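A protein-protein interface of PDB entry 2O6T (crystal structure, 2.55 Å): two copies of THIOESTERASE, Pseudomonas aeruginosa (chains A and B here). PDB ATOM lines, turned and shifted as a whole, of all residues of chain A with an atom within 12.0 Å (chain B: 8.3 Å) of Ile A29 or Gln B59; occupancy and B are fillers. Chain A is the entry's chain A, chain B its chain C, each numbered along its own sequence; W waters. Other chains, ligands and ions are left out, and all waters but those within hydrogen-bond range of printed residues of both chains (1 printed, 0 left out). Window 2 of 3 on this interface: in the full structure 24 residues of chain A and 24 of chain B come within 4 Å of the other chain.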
ATOM      1  N   ARG A  23      -3.655  16.466  26.382  1.00  0.00           N
ATOM      2  CA  ARG A  23      -3.524  15.649  27.542  1.00  0.00           C
ATOM      3  C   ARG A  23      -2.135  15.850  28.124  1.00  0.00           C
ATOM      4  O   ARG A  23      -1.172  16.169  27.367  1.00  0.00           O
ATOM      5  CB  ARG A  23      -3.741  14.208  27.127  1.00  0.00           C
ATOM      6  CG  ARG A  23      -5.221  13.798  26.998  1.00  0.00           C
ATOM      7  CD  ARG A  23      -5.367  12.346  26.704  1.00  0.00           C
ATOM      8  NE  ARG A  23      -6.627  12.058  26.053  1.00  0.00           N
ATOM      9  CZ  ARG A  23      -7.123  10.846  25.880  1.00  0.00           C
ATOM     10  NH1 ARG A  23      -6.466   9.793  26.354  1.00  0.00           N
ATOM     11  NH2 ARG A  23      -8.275  10.694  25.235  1.00  0.00           N
ATOM     12  N   TRP A  24      -2.005  15.710  29.450  1.00  0.00           N
ATOM     13  CA  TRP A  24      -0.718  15.930  30.107  1.00  0.00           C
ATOM     14  C   TRP A  24       0.475  15.315  29.335  1.00  0.00           C
ATOM     15  O   TRP A  24       1.478  15.956  29.008  1.00  0.00           O
ATOM     16  CB  TRP A  24      -0.721  15.345  31.506  1.00  0.00           C
ATOM     17  CG  TRP A  24       0.626  15.445  32.116  1.00  0.00           C
ATOM     18  CD1 TRP A  24       1.525  14.448  32.261  1.00  0.00           C
ATOM     19  CD2 TRP A  24       1.257  16.648  32.633  1.00  0.00           C
ATOM     20  NE1 TRP A  24       2.692  14.935  32.835  1.00  0.00           N
ATOM     21  CE2 TRP A  24       2.541  16.280  33.089  1.00  0.00           C
ATOM     22  CE3 TRP A  24       0.846  17.982  32.770  1.00  0.00           C
ATOM     23  CZ2 TRP A  24       3.443  17.215  33.649  1.00  0.00           C
ATOM     24  CZ3 TRP A  24       1.739  18.907  33.299  1.00  0.00           C
ATOM     25  CH2 TRP A  24       3.029  18.518  33.744  1.00  0.00           C
ATOM     26  N   HIS A  25       0.349  14.044  29.040  1.00  0.00           N
ATOM     27  CA  HIS A  25       1.452  13.299  28.528  1.00  0.00           C
ATOM     28  C   HIS A  25       1.509  13.398  27.039  1.00  0.00           C
ATOM     29  O   HIS A  25       2.247  12.646  26.418  1.00  0.00           O
ATOM     30  CB  HIS A  25       1.330  11.840  28.977  1.00  0.00           C
ATOM     31  CG  HIS A  25       2.615  11.093  28.941  1.00  0.00           C
ATOM     32  ND1 HIS A  25       2.689   9.730  29.150  1.00  0.00           N
ATOM     33  CD2 HIS A  25       3.886  11.518  28.736  1.00  0.00           C
ATOM     34  CE1 HIS A  25       3.952   9.351  29.075  1.00  0.00           C
ATOM     35  NE2 HIS A  25       4.698  10.418  28.828  1.00  0.00           N
ATOM     36  N   ASP A  26       0.758  14.312  26.436  1.00  0.00           N
ATOM     37  CA  ASP A  26       0.972  14.551  25.014  1.00  0.00           C
ATOM     38  C   ASP A  26       2.367  15.169  24.871  1.00  0.00           C
ATOM     39  O   ASP A  26       3.059  14.948  23.883  1.00  0.00           O
ATOM     40  CB  ASP A  26      -0.095  15.463  24.392  1.00  0.00           C
ATOM     41  CG  ASP A  26      -1.484  14.803  24.317  1.00  0.00           C
ATOM     42  OD1 ASP A  26      -1.567  13.543  24.342  1.00  0.00           O
ATOM     43  OD2 ASP A  26      -2.508  15.541  24.230  1.00  0.00           O
ATOM     44  N   ASN A  27       2.788  15.939  25.861  1.00  0.00           N
ATOM     45  CA  ASN A  27       4.080  16.601  25.792  1.00  0.00           C
ATOM     46  C   ASN A  27       5.108  15.556  26.117  1.00  0.00           C
ATOM     47  O   ASN A  27       4.911  14.739  27.033  1.00  0.00           O
ATOM     48  CB  ASN A  27       4.161  17.725  26.834  1.00  0.00           C
ATOM     49  CG  ASN A  27       3.332  18.940  26.464  1.00  0.00           C
ATOM     50  OD1 ASN A  27       3.061  19.170  25.309  1.00  0.00           O
ATOM     51  ND2 ASN A  27       2.922  19.698  27.446  1.00  0.00           N
ATOM     52  N   ASP A  28       6.198  15.535  25.359  1.00  0.00           N
ATOM     53  CA  ASP A  28       7.287  14.656  25.716  1.00  0.00           C
ATOM     54  C   ASP A  28       8.347  15.458  26.446  1.00  0.00           C
ATOM     55  O   ASP A  28       8.098  16.610  26.801  1.00  0.00           O
ATOM     56  CB  ASP A  28       7.817  13.875  24.507  1.00  0.00           C
ATOM     57  CG  ASP A  28       8.471  14.758  23.443  1.00  0.00           C
ATOM     58  OD1 ASP A  28       8.796  15.936  23.728  1.00  0.00           O
ATOM     59  OD2 ASP A  28       8.709  14.209  22.307  1.00  0.00           O
ATOM     60  N   ILE A  29       9.521  14.853  26.651  1.00  0.00           N
ATOM     61  CA  ILE A  29      10.570  15.445  27.398  1.00  0.00           C
ATOM     62  C   ILE A  29      11.072  16.795  26.828  1.00  0.00           C
ATOM     63  O   ILE A  29      11.597  17.634  27.570  1.00  0.00           O
ATOM     64  CB  ILE A  29      11.692  14.418  27.573  1.00  0.00           C
ATOM     65  CG1 ILE A  29      12.580  14.786  28.784  1.00  0.00           C
ATOM     66  CG2 ILE A  29      12.453  14.162  26.247  1.00  0.00           C
ATOM     67  CD1 ILE A  29      13.814  13.878  28.992  1.00  0.00           C
ATOM     68  N   TYR A  30      10.908  17.034  25.532  1.00  0.00           N
ATOM     69  CA  TYR A  30      11.339  18.307  24.966  1.00  0.00           C
ATOM     70  C   TYR A  30      10.251  19.366  25.130  1.00  0.00           C
ATOM     71  O   TYR A  30      10.468  20.528  24.801  1.00  0.00           O
ATOM     72  CB  TYR A  30      11.733  18.153  23.484  1.00  0.00           C
ATOM     73  CG  TYR A  30      12.954  17.246  23.255  1.00  0.00           C
ATOM     74  CD1 TYR A  30      14.017  17.193  24.189  1.00  0.00           C
ATOM     75  CD2 TYR A  30      13.049  16.457  22.100  1.00  0.00           C
ATOM     76  CE1 TYR A  30      15.121  16.387  23.982  1.00  0.00           C
ATOM     77  CE2 TYR A  30      14.190  15.654  21.864  1.00  0.00           C
ATOM     78  CZ  TYR A  30      15.201  15.615  22.830  1.00  0.00           C
ATOM     79  OH  TYR A  30      16.285  14.804  22.600  1.00  0.00           O
ATOM     80  N   GLY A  31       9.075  18.960  25.634  1.00  0.00           N
ATOM     81  CA  GLY A  31       8.068  19.908  26.147  1.00  0.00           C
ATOM     82  C   GLY A  31       6.911  20.271  25.227  1.00  0.00           C
ATOM     83  O   GLY A  31       6.020  21.031  25.629  1.00  0.00           O
ATOM     84  N   HIS A  32       6.915  19.745  23.999  1.00  0.00           N
ATOM     85  CA  HIS A  32       5.824  19.941  23.062  1.00  0.00           C
ATOM     86  C   HIS A  32       5.153  18.585  22.764  1.00  0.00           C
ATOM     87  O   HIS A  32       5.652  17.514  23.198  1.00  0.00           O
ATOM     88  CB  HIS A  32       6.351  20.598  21.792  1.00  0.00           C
ATOM     89  CG  HIS A  32       6.973  21.956  22.033  1.00  0.00           C
ATOM     90  ND1 HIS A  32       6.236  23.078  22.391  1.00  0.00           N
ATOM     91  CD2 HIS A  32       8.262  22.377  21.929  1.00  0.00           C
ATOM     92  CE1 HIS A  32       7.047  24.117  22.531  1.00  0.00           C
ATOM     93  NE2 HIS A  32       8.285  23.716  22.268  1.00  0.00           N
ATOM     94  N   VAL A  33       4.021  18.608  22.056  1.00  0.00           N
ATOM     95  CA  VAL A  33       3.343  17.367  21.779  1.00  0.00           C
ATOM     96  C   VAL A  33       4.262  16.502  20.942  1.00  0.00           C
ATOM     97  O   VAL A  33       4.783  16.950  19.930  1.00  0.00           O
ATOM     98  CB  VAL A  33       2.030  17.583  21.026  1.00  0.00           C
ATOM     99  CG1 VAL A  33       1.450  16.219  20.588  1.00  0.00           C
ATOM    100  CG2 VAL A  33       0.997  18.370  21.889  1.00  0.00           C
ATOM    101  N   ASN A  34       4.432  15.253  21.328  1.00  0.00           N
ATOM    102  CA  ASN A  34       5.224  14.294  20.561  1.00  0.00           C
ATOM    103  C   ASN A  34       4.707  14.043  19.138  1.00  0.00           C
ATOM    104  O   ASN A  34       3.515  14.053  18.919  1.00  0.00           O
ATOM    105  CB  ASN A  34       5.318  12.971  21.318  1.00  0.00           C
ATOM    106  CG  ASN A  34       6.203  11.974  20.607  1.00  0.00           C
ATOM    107  OD1 ASN A  34       5.716  10.976  20.048  1.00  0.00           O
ATOM    108  ND2 ASN A  34       7.492  12.271  20.557  1.00  0.00           N
ATOM    109  N   ASN A  35       5.592  13.800  18.173  1.00  0.00           N
ATOM    110  CA  ASN A  35       5.168  13.630  16.786  1.00  0.00           C
ATOM    111  C   ASN A  35       4.204  12.461  16.634  1.00  0.00           C
ATOM    112  O   ASN A  35       3.296  12.515  15.815  1.00  0.00           O
ATOM    113  CB  ASN A  35       6.378  13.426  15.864  1.00  0.00           C
ATOM    114  CG  ASN A  35       7.267  12.242  16.302  1.00  0.00           C
ATOM    115  OD1 ASN A  35       8.015  12.326  17.293  1.00  0.00           O
ATOM    116  ND2 ASN A  35       7.161  11.137  15.588  1.00  0.00           N
ATOM    117  N   VAL A  36       4.400  11.391  17.412  1.00  0.00           N
ATOM    118  CA  VAL A  36       3.545  10.224  17.267  1.00  0.00           C
ATOM    119  C   VAL A  36       2.114  10.556  17.569  1.00  0.00           C
ATOM    120  O   VAL A  36       1.223  10.110  16.846  1.00  0.00           O
ATOM    121  CB  VAL A  36       3.987   9.038  18.137  1.00  0.00           C
ATOM    122  CG1 VAL A  36       3.072   7.804  17.893  1.00  0.00           C
ATOM    123  CG2 VAL A  36       5.468   8.643  17.805  1.00  0.00           C
ATOM    124  N   THR A  37       1.874  11.352  18.618  1.00  0.00           N
ATOM    125  CA  THR A  37       0.522  11.750  18.994  1.00  0.00           C
ATOM    126  C   THR A  37      -0.296  12.387  17.841  1.00  0.00           C
ATOM    127  O   THR A  37      -1.522  12.223  17.758  1.00  0.00           O
ATOM    128  CB  THR A  37       0.591  12.654  20.202  1.00  0.00           C
ATOM    129  OG1 THR A  37       1.172  11.899  21.290  1.00  0.00           O
ATOM    130  CG2 THR A  37      -0.786  13.149  20.630  1.00  0.00           C
ATOM    131  N   PRO A  77       5.441  23.496  16.543  1.00  0.00           N
ATOM    132  CA  PRO A  77       5.033  22.613  17.654  1.00  0.00           C
ATOM    133  C   PRO A  77       3.782  23.122  18.351  1.00  0.00           C
ATOM    134  O   PRO A  77       3.511  24.308  18.224  1.00  0.00           O
ATOM    135  CB  PRO A  77       6.204  22.729  18.618  1.00  0.00           C
ATOM    136  CG  PRO A  77       6.693  24.150  18.386  1.00  0.00           C
ATOM    137  CD  PRO A  77       6.677  24.243  16.868  1.00  0.00           C
ATOM    138  N   VAL A  78       3.048  22.253  19.070  1.00  0.00           N
ATOM    139  CA  VAL A  78       2.051  22.712  19.988  1.00  0.00           C
ATOM    140  C   VAL A  78       2.308  21.994  21.269  1.00  0.00           C
ATOM    141  O   VAL A  78       3.101  21.054  21.275  1.00  0.00           O
ATOM    142  CB  VAL A  78       0.614  22.421  19.521  1.00  0.00           C
ATOM    143  CG1 VAL A  78       0.276  23.249  18.304  1.00  0.00           C
ATOM    144  CG2 VAL A  78       0.407  20.959  19.216  1.00  0.00           C
ATOM    145  N   ALA A  79       1.644  22.411  22.354  1.00  0.00           N
ATOM    146  CA  ALA A  79       1.882  21.868  23.688  1.00  0.00           C
ATOM    147  C   ALA A  79       0.578  21.792  24.496  1.00  0.00           C
ATOM    148  O   ALA A  79      -0.272  22.741  24.463  1.00  0.00           O
ATOM    149  CB  ALA A  79       2.898  22.717  24.443  1.00  0.00           C
ATOM    150  N   PHE A  80       0.433  20.691  25.248  1.00  0.00           N
ATOM    151  CA  PHE A  80      -0.538  20.666  26.330  1.00  0.00           C
ATOM    152  C   PHE A  80      -0.236  21.870  27.178  1.00  0.00           C
ATOM    153  O   PHE A  80       0.935  22.178  27.418  1.00  0.00           O
ATOM    154  CB  PHE A  80      -0.422  19.373  27.152  1.00  0.00           C
ATOM    155  CG  PHE A  80      -1.113  19.431  28.494  1.00  0.00           C
ATOM    156  CD1 PHE A  80      -2.429  18.995  28.625  1.00  0.00           C
ATOM    157  CD2 PHE A  80      -0.447  19.921  29.608  1.00  0.00           C
ATOM    158  CE1 PHE A  80      -3.069  19.030  29.823  1.00  0.00           C
ATOM    159  CE2 PHE A  80      -1.076  20.002  30.834  1.00  0.00           C
ATOM    160  CZ  PHE A  80      -2.399  19.562  30.984  1.00  0.00           C
ATOM    161  N   ASN B  47      16.102   7.198  18.773  1.00  0.00           N
ATOM    162  CA  ASN B  47      16.711   7.796  19.968  1.00  0.00           C
ATOM    163  C   ASN B  47      17.501   6.859  20.882  1.00  0.00           C
ATOM    164  O   ASN B  47      18.509   7.292  21.474  1.00  0.00           O
ATOM    165  CB  ASN B  47      15.714   8.628  20.756  1.00  0.00           C
ATOM    166  CG  ASN B  47      15.127   9.701  19.926  1.00  0.00           C
ATOM    167  OD1 ASN B  47      15.741  10.754  19.688  1.00  0.00           O
ATOM    168  ND2 ASN B  47      13.956   9.440  19.415  1.00  0.00           N
ATOM    169  N   ILE B  51      21.333   7.858  21.831  1.00  0.00           N
ATOM    170  CA  ILE B  51      21.859   7.899  23.176  1.00  0.00           C
ATOM    171  C   ILE B  51      23.006   6.900  23.425  1.00  0.00           C
ATOM    172  O   ILE B  51      24.033   7.277  23.982  1.00  0.00           O
ATOM    173  CB  ILE B  51      20.789   7.681  24.237  1.00  0.00           C
ATOM    174  CG1 ILE B  51      19.740   8.779  24.136  1.00  0.00           C
ATOM    175  CG2 ILE B  51      21.463   7.562  25.611  1.00  0.00           C
ATOM    176  CD1 ILE B  51      18.349   8.416  24.705  1.00  0.00           C
ATOM    177  N   LEU B  56      23.868  11.493  22.506  1.00  0.00           N
ATOM    178  CA  LEU B  56      22.670  12.295  22.778  1.00  0.00           C
ATOM    179  C   LEU B  56      22.385  12.419  24.309  1.00  0.00           C
ATOM    180  O   LEU B  56      22.363  11.414  25.047  1.00  0.00           O
ATOM    181  CB  LEU B  56      21.420  11.735  22.071  1.00  0.00           C
ATOM    182  CG  LEU B  56      20.230  12.689  22.163  1.00  0.00           C
ATOM    183  CD1 LEU B  56      20.556  14.012  21.437  1.00  0.00           C
ATOM    184  CD2 LEU B  56      18.932  12.147  21.656  1.00  0.00           C
ATOM    185  N   ASP B  57      22.186  13.650  24.777  1.00  0.00           N
ATOM    186  CA  ASP B  57      21.889  13.879  26.184  1.00  0.00           C
ATOM    187  C   ASP B  57      20.515  14.499  26.229  1.00  0.00           C
ATOM    188  O   ASP B  57      20.357  15.684  25.995  1.00  0.00           O
ATOM    189  CB  ASP B  57      22.937  14.783  26.826  1.00  0.00           C
ATOM    190  CG  ASP B  57      22.623  15.142  28.274  1.00  0.00           C
ATOM    191  OD1 ASP B  57      21.516  14.812  28.809  1.00  0.00           O
ATOM    192  OD2 ASP B  57      23.497  15.816  28.891  1.00  0.00           O
ATOM    193  N   ILE B  58      19.518  13.676  26.532  1.00  0.00           N
ATOM    194  CA  ILE B  58      18.148  14.111  26.456  1.00  0.00           C
ATOM    195  C   ILE B  58      17.770  14.918  27.682  1.00  0.00           C
ATOM    196  O   ILE B  58      16.872  15.755  27.636  1.00  0.00           O
ATOM    197  CB  ILE B  58      17.177  12.933  26.214  1.00  0.00           C
ATOM    198  CG1 ILE B  58      17.176  11.958  27.394  1.00  0.00           C
ATOM    199  CG2 ILE B  58      17.505  12.254  24.909  1.00  0.00           C
ATOM    200  CD1 ILE B  58      16.114  10.848  27.296  1.00  0.00           C
ATOM    201  N   GLN B  59      18.494  14.680  28.770  1.00  0.00           N
ATOM    202  CA  GLN B  59      18.177  15.296  30.045  1.00  0.00           C
ATOM    203  C   GLN B  59      18.645  16.720  30.066  1.00  0.00           C
ATOM    204  O   GLN B  59      17.876  17.600  30.455  1.00  0.00           O
ATOM    205  CB  GLN B  59      18.780  14.504  31.185  1.00  0.00           C
ATOM    206  CG  GLN B  59      18.248  13.084  31.264  1.00  0.00           C
ATOM    207  CD  GLN B  59      16.774  13.027  31.583  1.00  0.00           C
ATOM    208  OE1 GLN B  59      16.248  13.934  32.238  1.00  0.00           O
ATOM    209  NE2 GLN B  59      16.085  11.953  31.133  1.00  0.00           N
ATOM    210  N   GLY B  60      19.874  16.957  29.591  1.00  0.00           N
ATOM    211  CA  GLY B  60      20.509  18.298  29.661  1.00  0.00           C
ATOM    212  C   GLY B  60      21.324  18.771  28.440  1.00  0.00           C
ATOM    213  O   GLY B  60      21.990  19.808  28.507  1.00  0.00           O
ATOM    214  N   GLY B  61      21.261  18.025  27.332  1.00  0.00           N
ATOM    215  CA  GLY B  61      22.069  18.299  26.148  1.00  0.00           C
ATOM    216  C   GLY B  61      21.702  19.619  25.496  1.00  0.00           C
ATOM    217  O   GLY B  61      20.569  20.094  25.599  1.00  0.00           O
ATOM    218  N   GLU B  62      22.678  20.219  24.838  1.00  0.00           N
ATOM    219  CA  GLU B  62      22.510  21.510  24.197  1.00  0.00           C
ATOM    220  C   GLU B  62      21.784  21.340  22.858  1.00  0.00           C
ATOM    221  O   GLU B  62      21.003  22.208  22.450  1.00  0.00           O
ATOM    222  CB  GLU B  62      23.898  22.159  23.990  1.00  0.00           C
ATOM    223  CG  GLU B  62      23.988  23.624  24.403  1.00  0.00           C
ATOM    224  CD  GLU B  62      25.444  24.136  24.654  1.00  0.00           C
ATOM    225  OE1 GLU B  62      26.315  24.142  23.709  1.00  0.00           O
ATOM    226  OE2 GLU B  62      25.681  24.573  25.817  1.00  0.00           O
ATOM    227  N   ILE B  64      19.354  18.931  20.197  1.00  0.00           N
ATOM    228  CA  ILE B  64      18.331  17.863  20.104  1.00  0.00           C
ATOM    229  C   ILE B  64      17.787  17.617  18.687  1.00  0.00           C
ATOM    230  O   ILE B  64      17.883  18.465  17.771  1.00  0.00           O
ATOM    231  CB  ILE B  64      17.164  18.064  21.138  1.00  0.00           C
ATOM    232  CG1 ILE B  64      16.415  19.382  20.897  1.00  0.00           C
ATOM    233  CG2 ILE B  64      17.701  18.124  22.532  1.00  0.00           C
ATOM    234  CD1 ILE B  64      15.007  19.444  21.444  1.00  0.00           C
ATOM    235  N   ARG B 125      18.527  23.505  21.803  1.00  0.00           N
ATOM    236  CA  ARG B 125      17.389  23.267  22.672  1.00  0.00           C
ATOM    237  C   ARG B 125      16.686  24.533  23.173  1.00  0.00           C
ATOM    238  O   ARG B 125      15.451  24.577  23.210  1.00  0.00           O
ATOM    239  CB  ARG B 125      17.827  22.416  23.845  1.00  0.00           C
ATOM    240  CG  ARG B 125      16.725  21.682  24.558  1.00  0.00           C
ATOM    241  CD  ARG B 125      17.182  21.421  25.984  1.00  0.00           C
ATOM    242  NE  ARG B 125      16.285  20.482  26.689  1.00  0.00           N
ATOM    243  CZ  ARG B 125      16.541  19.189  26.870  1.00  0.00           C
ATOM    244  NH1 ARG B 125      17.683  18.636  26.391  1.00  0.00           N
ATOM    245  NH2 ARG B 125      15.643  18.467  27.532  1.00  0.00           N
HETATM  246  O   HOH W   1      16.228  13.858  20.050  1.00  0.00           O
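The backbone NH (N) of Tyr A30 is in hydrogen-bond range of the side-chain carboxylate (OD1) of Asp A28 (3.0 Å). OD1 of Asp B57 is in hydrogen-bond range of N of Gln B59. The backbone carbonyl oxygen (O) of Ile B58 lies within hydrogen-bond range of the guanidinium group (NH2) of Arg B125 (3.0 Å). The backbone carbonyl oxygen of Gly B61 sits at hydrogen-bond distance from the guanidinium group of Arg B125, at 3.3 Å. O of Glu B62 sits at hydrogen-bond distance from N of Arg B125 (2.9 Å).
Among the printed residues, merely in contact across the chains: Ile A29 with Ile B58, Ile A29 with Gln B59, Tyr A30 with Leu B56, Tyr A30 with Ile B58, Tyr A30 with Ile B64 and Tyr A30 with Arg B125.
Ile A29 touches just these residues of chain B: Ile B58 and Gln B59. Of chain A, only Ile A29 comes within 4 Å of Gln B59. No residue of chain A comes within 4 Å of Asp B57. Of chain A, only Ile A29 (3.8 Å) and Tyr A30 (3.6 Å) come within 4 Å of Ile B58. No residue of chain A comes within 4 Å of Gly B60. No residue of chain A comes within 4 Å of Gly B61. Printed residues of chain A within 4 Å of Arg B125: Tyr A30 (3.9 Å). Printed residues of chain A within 4 Å of Leu B56: Tyr A30 (3.9 Å). Of the printed residues of chain A, Ile B64 touches Tyr A30. Of the printed residues of chain B, Tyr A30 touches Leu B56 (3.9 Å), Ile B58 (3.6 Å), Ile B64 (3.4 Å) and Arg B125 (3.9 Å). The nearest residue of chain B that does not touch Ile A29 is Arg B125 (4.1 Å).
Of the 19 printed residues of chain A, 2 touch a printed residue of chain B. Hydrophobic or aromatic side chains of chain B that line the printed part of chain A: Leu B56, Ile B58 and Ile B64. Among the printed residues, 6 pairs touch across the chains.
No position is printed for both chains.
Water W1 lies within hydrogen-bond range of OH of Tyr A30 (2.7 Å) and OD1 of Asn B47 (3.2 Å).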
